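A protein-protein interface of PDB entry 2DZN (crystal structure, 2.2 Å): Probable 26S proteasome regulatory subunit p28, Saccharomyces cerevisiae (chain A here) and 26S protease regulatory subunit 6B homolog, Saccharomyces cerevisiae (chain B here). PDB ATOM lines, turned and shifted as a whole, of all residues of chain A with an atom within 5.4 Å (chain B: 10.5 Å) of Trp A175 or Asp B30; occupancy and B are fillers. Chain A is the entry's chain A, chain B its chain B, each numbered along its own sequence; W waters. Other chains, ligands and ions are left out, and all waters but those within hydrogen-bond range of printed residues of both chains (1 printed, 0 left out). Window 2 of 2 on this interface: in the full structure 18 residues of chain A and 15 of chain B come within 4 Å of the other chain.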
ATOM      1  N   HIS A 145       8.609  -6.006  20.612  1.00  0.00           N
ATOM      2  CA  HIS A 145       8.571  -7.328  19.993  1.00  0.00           C
ATOM      3  C   HIS A 145       8.903  -8.381  21.059  1.00  0.00           C
ATOM      4  O   HIS A 145       8.310  -9.472  21.072  1.00  0.00           O
ATOM      5  CB  HIS A 145       9.576  -7.460  18.832  1.00  0.00           C
ATOM      6  CG  HIS A 145       9.094  -6.884  17.532  1.00  0.00           C
ATOM      7  ND1 HIS A 145       9.384  -5.596  17.136  1.00  0.00           N
ATOM      8  CD2 HIS A 145       8.329  -7.416  16.550  1.00  0.00           C
ATOM      9  CE1 HIS A 145       8.816  -5.360  15.966  1.00  0.00           C
ATOM     10  NE2 HIS A 145       8.170  -6.448  15.587  1.00  0.00           N
ATOM     11  N   TRP A 169       5.134  -2.039  13.697  1.00  0.00           N
ATOM     12  CA  TRP A 169       6.382  -2.302  12.985  1.00  0.00           C
ATOM     13  C   TRP A 169       6.571  -3.787  12.811  1.00  0.00           C
ATOM     14  O   TRP A 169       6.338  -4.565  13.740  1.00  0.00           O
ATOM     15  CB  TRP A 169       7.555  -1.707  13.748  1.00  0.00           C
ATOM     16  CG  TRP A 169       7.591  -0.220  13.665  1.00  0.00           C
ATOM     17  CD1 TRP A 169       6.631   0.596  13.126  1.00  0.00           C
ATOM     18  CD2 TRP A 169       8.626   0.641  14.149  1.00  0.00           C
ATOM     19  NE1 TRP A 169       7.005   1.908  13.250  1.00  0.00           N
ATOM     20  CE2 TRP A 169       8.226   1.967  13.875  1.00  0.00           C
ATOM     21  CE3 TRP A 169       9.855   0.419  14.789  1.00  0.00           C
ATOM     22  CZ2 TRP A 169       9.008   3.073  14.225  1.00  0.00           C
ATOM     23  CZ3 TRP A 169      10.636   1.514  15.138  1.00  0.00           C
ATOM     24  CH2 TRP A 169      10.211   2.828  14.856  1.00  0.00           C
ATOM     25  N   GLN A 170       6.987  -4.181  11.617  1.00  0.00           N
ATOM     26  CA  GLN A 170       7.174  -5.592  11.312  1.00  0.00           C
ATOM     27  C   GLN A 170       8.656  -5.942  11.311  1.00  0.00           C
ATOM     28  O   GLN A 170       9.483  -5.132  10.892  1.00  0.00           O
ATOM     29  CB  GLN A 170       6.547  -5.908   9.943  1.00  0.00           C
ATOM     30  CG  GLN A 170       5.038  -5.659   9.896  1.00  0.00           C
ATOM     31  CD  GLN A 170       4.402  -5.963   8.540  1.00  0.00           C
ATOM     32  OE1 GLN A 170       4.162  -7.120   8.191  1.00  0.00           O
ATOM     33  NE2 GLN A 170       4.129  -4.916   7.772  1.00  0.00           N
ATOM     34  N   ASP A 171       8.999  -7.139  11.782  1.00  0.00           N
ATOM     35  CA  ASP A 171      10.407  -7.544  11.818  1.00  0.00           C
ATOM     36  C   ASP A 171      10.853  -8.248  10.527  1.00  0.00           C
ATOM     37  O   ASP A 171      10.054  -8.400   9.602  1.00  0.00           O
ATOM     38  CB  ASP A 171      10.699  -8.407  13.070  1.00  0.00           C
ATOM     39  CG  ASP A 171       9.996  -9.764  13.055  1.00  0.00           C
ATOM     40  OD1 ASP A 171       9.569 -10.220  11.980  1.00  0.00           O
ATOM     41  OD2 ASP A 171       9.896 -10.392  14.131  1.00  0.00           O
ATOM     42  N   GLN A 173      11.099 -11.054   9.684  1.00  0.00           N
ATOM     43  CA  GLN A 173      10.276 -12.208   9.435  1.00  0.00           C
ATOM     44  C   GLN A 173       8.869 -11.764   9.017  1.00  0.00           C
ATOM     45  O   GLN A 173       8.045 -12.569   8.574  1.00  0.00           O
ATOM     46  CB  GLN A 173      10.273 -13.004  10.735  1.00  0.00           C
ATOM     47  CG  GLN A 173       9.351 -14.164  10.856  1.00  0.00           C
ATOM     48  CD  GLN A 173       9.395 -14.753  12.271  1.00  0.00           C
ATOM     49  OE1 GLN A 173       8.892 -15.851  12.506  1.00  0.00           O
ATOM     50  NE2 GLN A 173       9.992 -14.014  13.218  1.00  0.00           N
ATOM     51  N   GLY A 174       8.603 -10.471   9.151  1.00  0.00           N
ATOM     52  CA  GLY A 174       7.300  -9.947   8.798  1.00  0.00           C
ATOM     53  C   GLY A 174       6.337  -9.907   9.972  1.00  0.00           C
ATOM     54  O   GLY A 174       5.147  -9.680   9.791  1.00  0.00           O
ATOM     55  N   TRP A 175       6.848 -10.092  11.181  1.00  0.00           N
ATOM     56  CA  TRP A 175       6.002 -10.096  12.366  1.00  0.00           C
ATOM     57  C   TRP A 175       5.963  -8.799  13.149  1.00  0.00           C
ATOM     58  O   TRP A 175       6.995  -8.197  13.436  1.00  0.00           O
ATOM     59  CB  TRP A 175       6.448 -11.213  13.324  1.00  0.00           C
ATOM     60  CG  TRP A 175       6.159 -12.619  12.861  1.00  0.00           C
ATOM     61  CD1 TRP A 175       5.913 -13.034  11.580  1.00  0.00           C
ATOM     62  CD2 TRP A 175       6.130 -13.803  13.676  1.00  0.00           C
ATOM     63  NE1 TRP A 175       5.737 -14.396  11.549  1.00  0.00           N
ATOM     64  CE2 TRP A 175       5.862 -14.894  12.819  1.00  0.00           C
ATOM     65  CE3 TRP A 175       6.308 -14.047  15.047  1.00  0.00           C
ATOM     66  CZ2 TRP A 175       5.758 -16.213  13.289  1.00  0.00           C
ATOM     67  CZ3 TRP A 175       6.207 -15.351  15.518  1.00  0.00           C
ATOM     68  CH2 TRP A 175       5.934 -16.420  14.639  1.00  0.00           C
ATOM     69  N   THR A 176       4.763  -8.365  13.486  1.00  0.00           N
ATOM     70  CA  THR A 176       4.594  -7.187  14.337  1.00  0.00           C
ATOM     71  C   THR A 176       4.626  -7.796  15.758  1.00  0.00           C
ATOM     72  O   THR A 176       4.661  -9.026  15.920  1.00  0.00           O
ATOM     73  CB  THR A 176       3.198  -6.548  14.189  1.00  0.00           C
ATOM     74  OG1 THR A 176       2.210  -7.506  14.598  1.00  0.00           O
ATOM     75  CG2 THR A 176       2.941  -6.119  12.759  1.00  0.00           C
ATOM     76  N   PRO A 177       4.615  -6.958  16.802  1.00  0.00           N
ATOM     77  CA  PRO A 177       4.634  -7.590  18.123  1.00  0.00           C
ATOM     78  C   PRO A 177       3.431  -8.546  18.323  1.00  0.00           C
ATOM     79  O   PRO A 177       3.579  -9.590  18.943  1.00  0.00           O
ATOM     80  CB  PRO A 177       4.622  -6.390  19.065  1.00  0.00           C
ATOM     81  CG  PRO A 177       5.461  -5.385  18.307  1.00  0.00           C
ATOM     82  CD  PRO A 177       4.869  -5.508  16.906  1.00  0.00           C
ATOM     83  N   PHE A 179       1.965 -10.569  16.270  1.00  0.00           N
ATOM     84  CA  PHE A 179       2.334 -11.861  15.735  1.00  0.00           C
ATOM     85  C   PHE A 179       3.086 -12.680  16.801  1.00  0.00           C
ATOM     86  O   PHE A 179       2.905 -13.900  16.919  1.00  0.00           O
ATOM     87  CB  PHE A 179       3.265 -11.672  14.546  1.00  0.00           C
ATOM     88  CG  PHE A 179       2.581 -11.672  13.228  1.00  0.00           C
ATOM     89  CD1 PHE A 179       2.677 -12.774  12.393  1.00  0.00           C
ATOM     90  CD2 PHE A 179       1.859 -10.565  12.806  1.00  0.00           C
ATOM     91  CE1 PHE A 179       2.055 -12.785  11.157  1.00  0.00           C
ATOM     92  CE2 PHE A 179       1.231 -10.565  11.571  1.00  0.00           C
ATOM     93  CZ  PHE A 179       1.332 -11.673  10.741  1.00  0.00           C
ATOM     94  N   HIS A 180       3.941 -12.003  17.563  1.00  0.00           N
ATOM     95  CA  HIS A 180       4.759 -12.678  18.567  1.00  0.00           C
ATOM     96  C   HIS A 180       3.962 -13.184  19.752  1.00  0.00           C
ATOM     97  O   HIS A 180       4.194 -14.310  20.203  1.00  0.00           O
ATOM     98  CB  HIS A 180       5.902 -11.751  19.038  1.00  0.00           C
ATOM     99  CG  HIS A 180       7.051 -11.672  18.075  1.00  0.00           C
ATOM    100  ND1 HIS A 180       8.090 -12.576  18.081  1.00  0.00           N
ATOM    101  CD2 HIS A 180       7.287 -10.837  17.035  1.00  0.00           C
ATOM    102  CE1 HIS A 180       8.914 -12.307  17.082  1.00  0.00           C
ATOM    103  NE2 HIS A 180       8.449 -11.257  16.430  1.00  0.00           N
ATOM    104  N   ALA A 183       1.934 -16.232  18.587  1.00  0.00           N
ATOM    105  CA  ALA A 183       2.758 -17.395  18.281  1.00  0.00           C
ATOM    106  C   ALA A 183       3.188 -18.096  19.575  1.00  0.00           C
ATOM    107  O   ALA A 183       3.481 -19.296  19.582  1.00  0.00           O
ATOM    108  CB  ALA A 183       3.988 -16.973  17.482  1.00  0.00           C
ATOM    109  N   GLU A 184       3.212 -17.344  20.671  1.00  0.00           N
ATOM    110  CA  GLU A 184       3.628 -17.891  21.949  1.00  0.00           C
ATOM    111  C   GLU A 184       2.501 -18.153  22.938  1.00  0.00           C
ATOM    112  O   GLU A 184       2.742 -18.365  24.130  1.00  0.00           O
ATOM    113  CB  GLU A 184       4.683 -16.981  22.569  1.00  0.00           C
ATOM    114  CG  GLU A 184       6.004 -17.089  21.850  1.00  0.00           C
ATOM    115  CD  GLU A 184       7.181 -17.123  22.808  1.00  0.00           C
ATOM    116  OE1 GLU A 184       7.050 -17.735  23.892  1.00  0.00           O
ATOM    117  OE2 GLU A 184       8.240 -16.552  22.473  1.00  0.00           O
ATOM    118  N   ASP A 205       2.643 -11.637   7.230  1.00  0.00           N
ATOM    119  CA  ASP A 205       4.086 -11.846   7.285  1.00  0.00           C
ATOM    120  C   ASP A 205       4.625 -12.270   5.926  1.00  0.00           C
ATOM    121  O   ASP A 205       3.883 -12.315   4.942  1.00  0.00           O
ATOM    122  CB  ASP A 205       4.444 -12.885   8.360  1.00  0.00           C
ATOM    123  CG  ASP A 205       4.062 -14.302   7.974  1.00  0.00           C
ATOM    124  OD1 ASP A 205       4.182 -15.201   8.838  1.00  0.00           O
ATOM    125  OD2 ASP A 205       3.657 -14.527   6.815  1.00  0.00           O
ATOM    126  N   VAL A 214      -0.746 -17.509  12.950  1.00  0.00           N
ATOM    127  CA  VAL A 214       0.486 -18.049  13.531  1.00  0.00           C
ATOM    128  C   VAL A 214       0.278 -18.368  15.002  1.00  0.00           C
ATOM    129  O   VAL A 214       1.249 -18.594  15.729  1.00  0.00           O
ATOM    130  CB  VAL A 214       1.693 -17.069  13.444  1.00  0.00           C
ATOM    131  CG1 VAL A 214       1.922 -16.632  12.025  1.00  0.00           C
ATOM    132  CG2 VAL A 214       1.470 -15.889  14.331  1.00  0.00           C
ATOM    133  N   LEU B  22      19.567 -16.225  25.461  1.00  0.00           N
ATOM    134  CA  LEU B  22      19.243 -17.304  24.536  1.00  0.00           C
ATOM    135  C   LEU B  22      17.857 -17.075  23.943  1.00  0.00           C
ATOM    136  O   LEU B  22      17.616 -17.364  22.768  1.00  0.00           O
ATOM    137  CB  LEU B  22      19.267 -18.643  25.260  1.00  0.00           C
ATOM    138  CG  LEU B  22      18.812 -19.875  24.484  1.00  0.00           C
ATOM    139  CD1 LEU B  22      19.692 -20.120  23.294  1.00  0.00           C
ATOM    140  CD2 LEU B  22      18.869 -21.065  25.407  1.00  0.00           C
ATOM    141  N   ASP B  23      16.947 -16.569  24.765  1.00  0.00           N
ATOM    142  CA  ASP B  23      15.593 -16.274  24.297  1.00  0.00           C
ATOM    143  C   ASP B  23      15.653 -14.958  23.508  1.00  0.00           C
ATOM    144  O   ASP B  23      14.969 -13.978  23.814  1.00  0.00           O
ATOM    145  CB  ASP B  23      14.617 -16.153  25.483  1.00  0.00           C
ATOM    146  CG  ASP B  23      14.339 -17.497  26.162  1.00  0.00           C
ATOM    147  OD1 ASP B  23      13.906 -18.440  25.462  1.00  0.00           O
ATOM    148  OD2 ASP B  23      14.546 -17.609  27.395  1.00  0.00           O
ATOM    149  N   SER B  24      16.511 -14.953  22.500  1.00  0.00           N
ATOM    150  CA  SER B  24      16.713 -13.815  21.616  1.00  0.00           C
ATOM    151  C   SER B  24      16.941 -14.460  20.261  1.00  0.00           C
ATOM    152  O   SER B  24      16.522 -13.949  19.230  1.00  0.00           O
ATOM    153  CB  SER B  24      17.958 -13.021  22.038  1.00  0.00           C
ATOM    154  OG  SER B  24      18.701 -12.535  20.918  1.00  0.00           O
ATOM    155  N   LEU B  25      17.611 -15.603  20.280  1.00  0.00           N
ATOM    156  CA  LEU B  25      17.884 -16.330  19.056  1.00  0.00           C
ATOM    157  C   LEU B  25      16.605 -17.012  18.598  1.00  0.00           C
ATOM    158  O   LEU B  25      16.385 -17.216  17.404  1.00  0.00           O
ATOM    159  CB  LEU B  25      18.948 -17.398  19.287  1.00  0.00           C
ATOM    160  CG  LEU B  25      20.208 -17.013  20.046  1.00  0.00           C
ATOM    161  CD1 LEU B  25      21.152 -18.222  20.081  1.00  0.00           C
ATOM    162  CD2 LEU B  25      20.848 -15.817  19.388  1.00  0.00           C
ATOM    163  N   ILE B  26      15.756 -17.356  19.554  1.00  0.00           N
ATOM    164  CA  ILE B  26      14.514 -18.051  19.251  1.00  0.00           C
ATOM    165  C   ILE B  26      13.430 -17.177  18.628  1.00  0.00           C
ATOM    166  O   ILE B  26      12.662 -17.642  17.789  1.00  0.00           O
ATOM    167  CB  ILE B  26      13.946 -18.701  20.532  1.00  0.00           C
ATOM    168  CG1 ILE B  26      13.814 -17.641  21.634  1.00  0.00           C
ATOM    169  CG2 ILE B  26      14.875 -19.817  21.001  1.00  0.00           C
ATOM    170  CD1 ILE B  26      12.935 -18.062  22.800  1.00  0.00           C
ATOM    171  N   ILE B  27      13.398 -15.911  19.039  1.00  0.00           N
ATOM    172  CA  ILE B  27      12.415 -14.906  18.612  1.00  0.00           C
ATOM    173  C   ILE B  27      12.537 -14.422  17.167  1.00  0.00           C
ATOM    174  O   ILE B  27      11.654 -13.732  16.657  1.00  0.00           O
ATOM    175  CB  ILE B  27      12.494 -13.680  19.590  1.00  0.00           C
ATOM    176  CG1 ILE B  27      11.907 -14.079  20.936  1.00  0.00           C
ATOM    177  CG2 ILE B  27      11.779 -12.477  19.057  1.00  0.00           C
ATOM    178  CD1 ILE B  27      10.659 -14.934  20.813  1.00  0.00           C
ATOM    179  N   ARG B  28      13.619 -14.820  16.508  1.00  0.00           N
ATOM    180  CA  ARG B  28      13.910 -14.383  15.151  1.00  0.00           C
ATOM    181  C   ARG B  28      13.098 -14.925  14.008  1.00  0.00           C
ATOM    182  O   ARG B  28      12.356 -14.184  13.373  1.00  0.00           O
ATOM    183  CB  ARG B  28      15.384 -14.606  14.870  1.00  0.00           C
ATOM    184  CG  ARG B  28      16.209 -13.708  15.720  1.00  0.00           C
ATOM    185  CD  ARG B  28      17.637 -14.121  15.755  1.00  0.00           C
ATOM    186  NE  ARG B  28      18.314 -13.406  16.823  1.00  0.00           N
ATOM    187  CZ  ARG B  28      19.621 -13.443  17.024  1.00  0.00           C
ATOM    188  NH1 ARG B  28      20.390 -14.165  16.219  1.00  0.00           N
ATOM    189  NH2 ARG B  28      20.142 -12.761  18.030  1.00  0.00           N
ATOM    190  N   ASN B  29      13.258 -16.202  13.716  1.00  0.00           N
ATOM    191  CA  ASN B  29      12.522 -16.800  12.625  1.00  0.00           C
ATOM    192  C   ASN B  29      11.860 -18.026  13.192  1.00  0.00           C
ATOM    193  O   ASN B  29      12.106 -19.141  12.741  1.00  0.00           O
ATOM    194  CB  ASN B  29      13.469 -17.186  11.497  1.00  0.00           C
ATOM    195  CG  ASN B  29      14.529 -18.154  11.949  1.00  0.00           C
ATOM    196  OD1 ASN B  29      15.393 -17.813  12.757  1.00  0.00           O
ATOM    197  ND2 ASN B  29      14.463 -19.378  11.441  1.00  0.00           N
ATOM    198  N   ASP B  30      11.022 -17.797  14.197  1.00  0.00           N
ATOM    199  CA  ASP B  30      10.307 -18.868  14.877  1.00  0.00           C
ATOM    200  C   ASP B  30      10.018 -20.060  13.969  1.00  0.00           C
ATOM    201  O   ASP B  30       9.743 -19.903  12.771  1.00  0.00           O
ATOM    202  CB  ASP B  30       9.003 -18.342  15.507  1.00  0.00           C
ATOM    203  CG  ASP B  30       9.256 -17.416  16.700  1.00  0.00           C
ATOM    204  OD1 ASP B  30       8.518 -17.507  17.711  1.00  0.00           O
ATOM    205  OD2 ASP B  30      10.192 -16.591  16.625  1.00  0.00           O
ATOM    206  N   SER B  31      10.105 -21.241  14.580  1.00  0.00           N
ATOM    207  CA  SER B  31       9.899 -22.545  13.952  1.00  0.00           C
ATOM    208  C   SER B  31      11.228 -23.249  13.696  1.00  0.00           C
ATOM    209  O   SER B  31      11.524 -23.681  12.579  1.00  0.00           O
ATOM    210  CB  SER B  31       9.093 -22.440  12.649  1.00  0.00           C
ATOM    211  OG  SER B  31       7.697 -22.443  12.918  1.00  0.00           O
ATOM    212  N   LEU B  32      12.029 -23.345  14.755  1.00  0.00           N
ATOM    213  CA  LEU B  32      13.316 -24.024  14.688  1.00  0.00           C
ATOM    214  C   LEU B  32      13.138 -25.371  15.371  1.00  0.00           C
ATOM    215  O   LEU B  32      12.632 -25.434  16.496  1.00  0.00           O
ATOM    216  CB  LEU B  32      14.399 -23.233  15.424  1.00  0.00           C
ATOM    217  CG  LEU B  32      14.841 -21.881  14.870  1.00  0.00           C
ATOM    218  CD1 LEU B  32      16.180 -21.528  15.483  1.00  0.00           C
ATOM    219  CD2 LEU B  32      14.959 -21.940  13.352  1.00  0.00           C
ATOM    220  N   SER B  33      13.534 -26.448  14.698  1.00  0.00           N
ATOM    221  CA  SER B  33      13.403 -27.770  15.289  1.00  0.00           C
ATOM    222  C   SER B  33      14.202 -27.790  16.589  1.00  0.00           C
ATOM    223  O   SER B  33      15.051 -26.926  16.811  1.00  0.00           O
ATOM    224  CB  SER B  33      13.924 -28.845  14.327  1.00  0.00           C
ATOM    225  OG  SER B  33      15.300 -28.672  14.049  1.00  0.00           O
ATOM    226  N   GLY B  34      13.916 -28.751  17.459  1.00  0.00           N
ATOM    227  CA  GLY B  34      14.659 -28.838  18.703  1.00  0.00           C
ATOM    228  C   GLY B  34      16.105 -29.135  18.347  1.00  0.00           C
ATOM    229  O   GLY B  34      17.034 -28.600  18.952  1.00  0.00           O
ATOM    230  N   VAL B  36      18.005 -28.232  15.827  1.00  0.00           N
ATOM    231  CA  VAL B  36      18.757 -27.025  15.526  1.00  0.00           C
ATOM    232  C   VAL B  36      19.120 -26.274  16.805  1.00  0.00           C
ATOM    233  O   VAL B  36      20.240 -25.791  16.952  1.00  0.00           O
ATOM    234  CB  VAL B  36      17.941 -26.106  14.580  1.00  0.00           C
ATOM    235  CG1 VAL B  36      18.689 -24.819  14.313  1.00  0.00           C
ATOM    236  CG2 VAL B  36      17.674 -26.843  13.258  1.00  0.00           C
ATOM    237  N   ILE B  37      18.178 -26.183  17.738  1.00  0.00           N
ATOM    238  CA  ILE B  37      18.438 -25.488  18.992  1.00  0.00           C
ATOM    239  C   ILE B  37      19.576 -26.178  19.742  1.00  0.00           C
ATOM    240  O   ILE B  37      20.448 -25.515  20.323  1.00  0.00           O
ATOM    241  CB  ILE B  37      17.174 -25.434  19.874  1.00  0.00           C
ATOM    242  CG1 ILE B  37      16.237 -24.352  19.339  1.00  0.00           C
ATOM    243  CG2 ILE B  37      17.541 -25.148  21.325  1.00  0.00           C
ATOM    244  CD1 ILE B  37      14.952 -24.248  20.081  1.00  0.00           C
ATOM    245  N   TYR B  65      24.468 -19.555  16.210  1.00  0.00           N
ATOM    246  CA  TYR B  65      23.256 -19.388  15.423  1.00  0.00           C
ATOM    247  C   TYR B  65      23.604 -19.017  13.971  1.00  0.00           C
ATOM    248  O   TYR B  65      23.029 -19.557  13.017  1.00  0.00           O
ATOM    249  CB  TYR B  65      22.419 -18.286  16.061  1.00  0.00           C
ATOM    250  CG  TYR B  65      21.180 -17.872  15.306  1.00  0.00           C
ATOM    251  CD1 TYR B  65      19.991 -18.591  15.424  1.00  0.00           C
ATOM    252  CD2 TYR B  65      21.186 -16.729  14.502  1.00  0.00           C
ATOM    253  CE1 TYR B  65      18.829 -18.180  14.767  1.00  0.00           C
ATOM    254  CE2 TYR B  65      20.036 -16.311  13.838  1.00  0.00           C
ATOM    255  CZ  TYR B  65      18.861 -17.042  13.976  1.00  0.00           C
ATOM    256  OH  TYR B  65      17.731 -16.625  13.324  1.00  0.00           O
ATOM    257  N   VAL B  69      21.535 -22.044  11.217  1.00  0.00           N
ATOM    258  CA  VAL B  69      20.244 -21.685  10.653  1.00  0.00           C
ATOM    259  C   VAL B  69      20.164 -21.853   9.135  1.00  0.00           C
ATOM    260  O   VAL B  69      19.529 -22.797   8.647  1.00  0.00           O
ATOM    261  CB  VAL B  69      19.883 -20.240  11.033  1.00  0.00           C
ATOM    262  CG1 VAL B  69      18.492 -19.887  10.524  1.00  0.00           C
ATOM    263  CG2 VAL B  69      19.948 -20.093  12.531  1.00  0.00           C
HETATM  264  O   HOH W   1       8.111 -15.363  19.243  1.00  0.00           O
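The side-chain hydroxyl of Tyr B65 lies within hydrogen-bond range of the side-chain amide oxygen of Asn B29, 2.7 Å away.
The side-chain carboxylate (OD2) of Asp A171 is in hydrogen-bond range of a ring nitrogen (NE2) of His A180 (2.9 Å).
NE1 of Trp A175 sits at hydrogen-bond distance from OD1 of Asp A205 (3.2 Å).
NE2 of His A145 lies within hydrogen-bond range of O of Trp A175 (3.0 Å).
O of Ser B24 sits at hydrogen-bond distance from NE of Arg B28.
The backbone NH (N) of Gln A173 lies within hydrogen-bond range of the side-chain carboxylate (OD1) of Asp A171.
Ile B27 touches Gln A173 (O to NE2, 3.8 Å).
Asn B29 touches Gln A173.
CB of Asp B30 touches CH2 of Trp A175, 3.7 Å away.
His A180 touches Ile B27 (CE1 to O, 3.1 Å).
OE2 of Glu A184 touches CD1 of Ile B27, at 3.4 Å.
The side-chain amide nitrogen of Gln A173 sits close to the backbone carbonyl oxygen of Arg B28, 2.4 Å away.
OE1 of Gln A173 lies within hydrogen-bond range of N of Asp B30, 3.3 Å away.
Trp A175 touches one residue of chain B.
No residue of chain B comes within 4 Å of Asp A171.
No residue of chain B comes within 4 Å of Gly A174.
No residue of chain B comes within 4 Å of Pro A177.
No residue of chain B comes within 4 Å of Phe A179.
His A180 touches one residue of chain B.
No residue of chain B comes within 4 Å of Ala A183.
Printed residues of chain B within 4 Å of Glu A184: Ile B27.
Of the printed residues of chain A, Arg B28 touches Gln A173.
Of the printed residues of chain A, Ile B27 touches Gln A173 (3.8 Å), His A180 (3.1 Å) and Glu A184 (3.4 Å).
Printed residues of chain A within 4 Å of Asn B29: Gln A173 (3.7 Å).
The nearest printed residue of chain A that does not touch Ile B27 is Asp A171 (4.5 Å).
Water W1 lies within hydrogen-bond range of the side-chain carboxylate (OD1) of Asp B30 (2.7 Å), a ring nitrogen (ND1) of His A180 (3.0 Å) and the side-chain carboxylate (OE2) of Glu A184 (3.4 Å).
Hydrophobic or aromatic side chains of chain A that line the printed part of chain B: Trp A175 and His A180.
Among the printed residues, 7 pairs touch across the chains.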
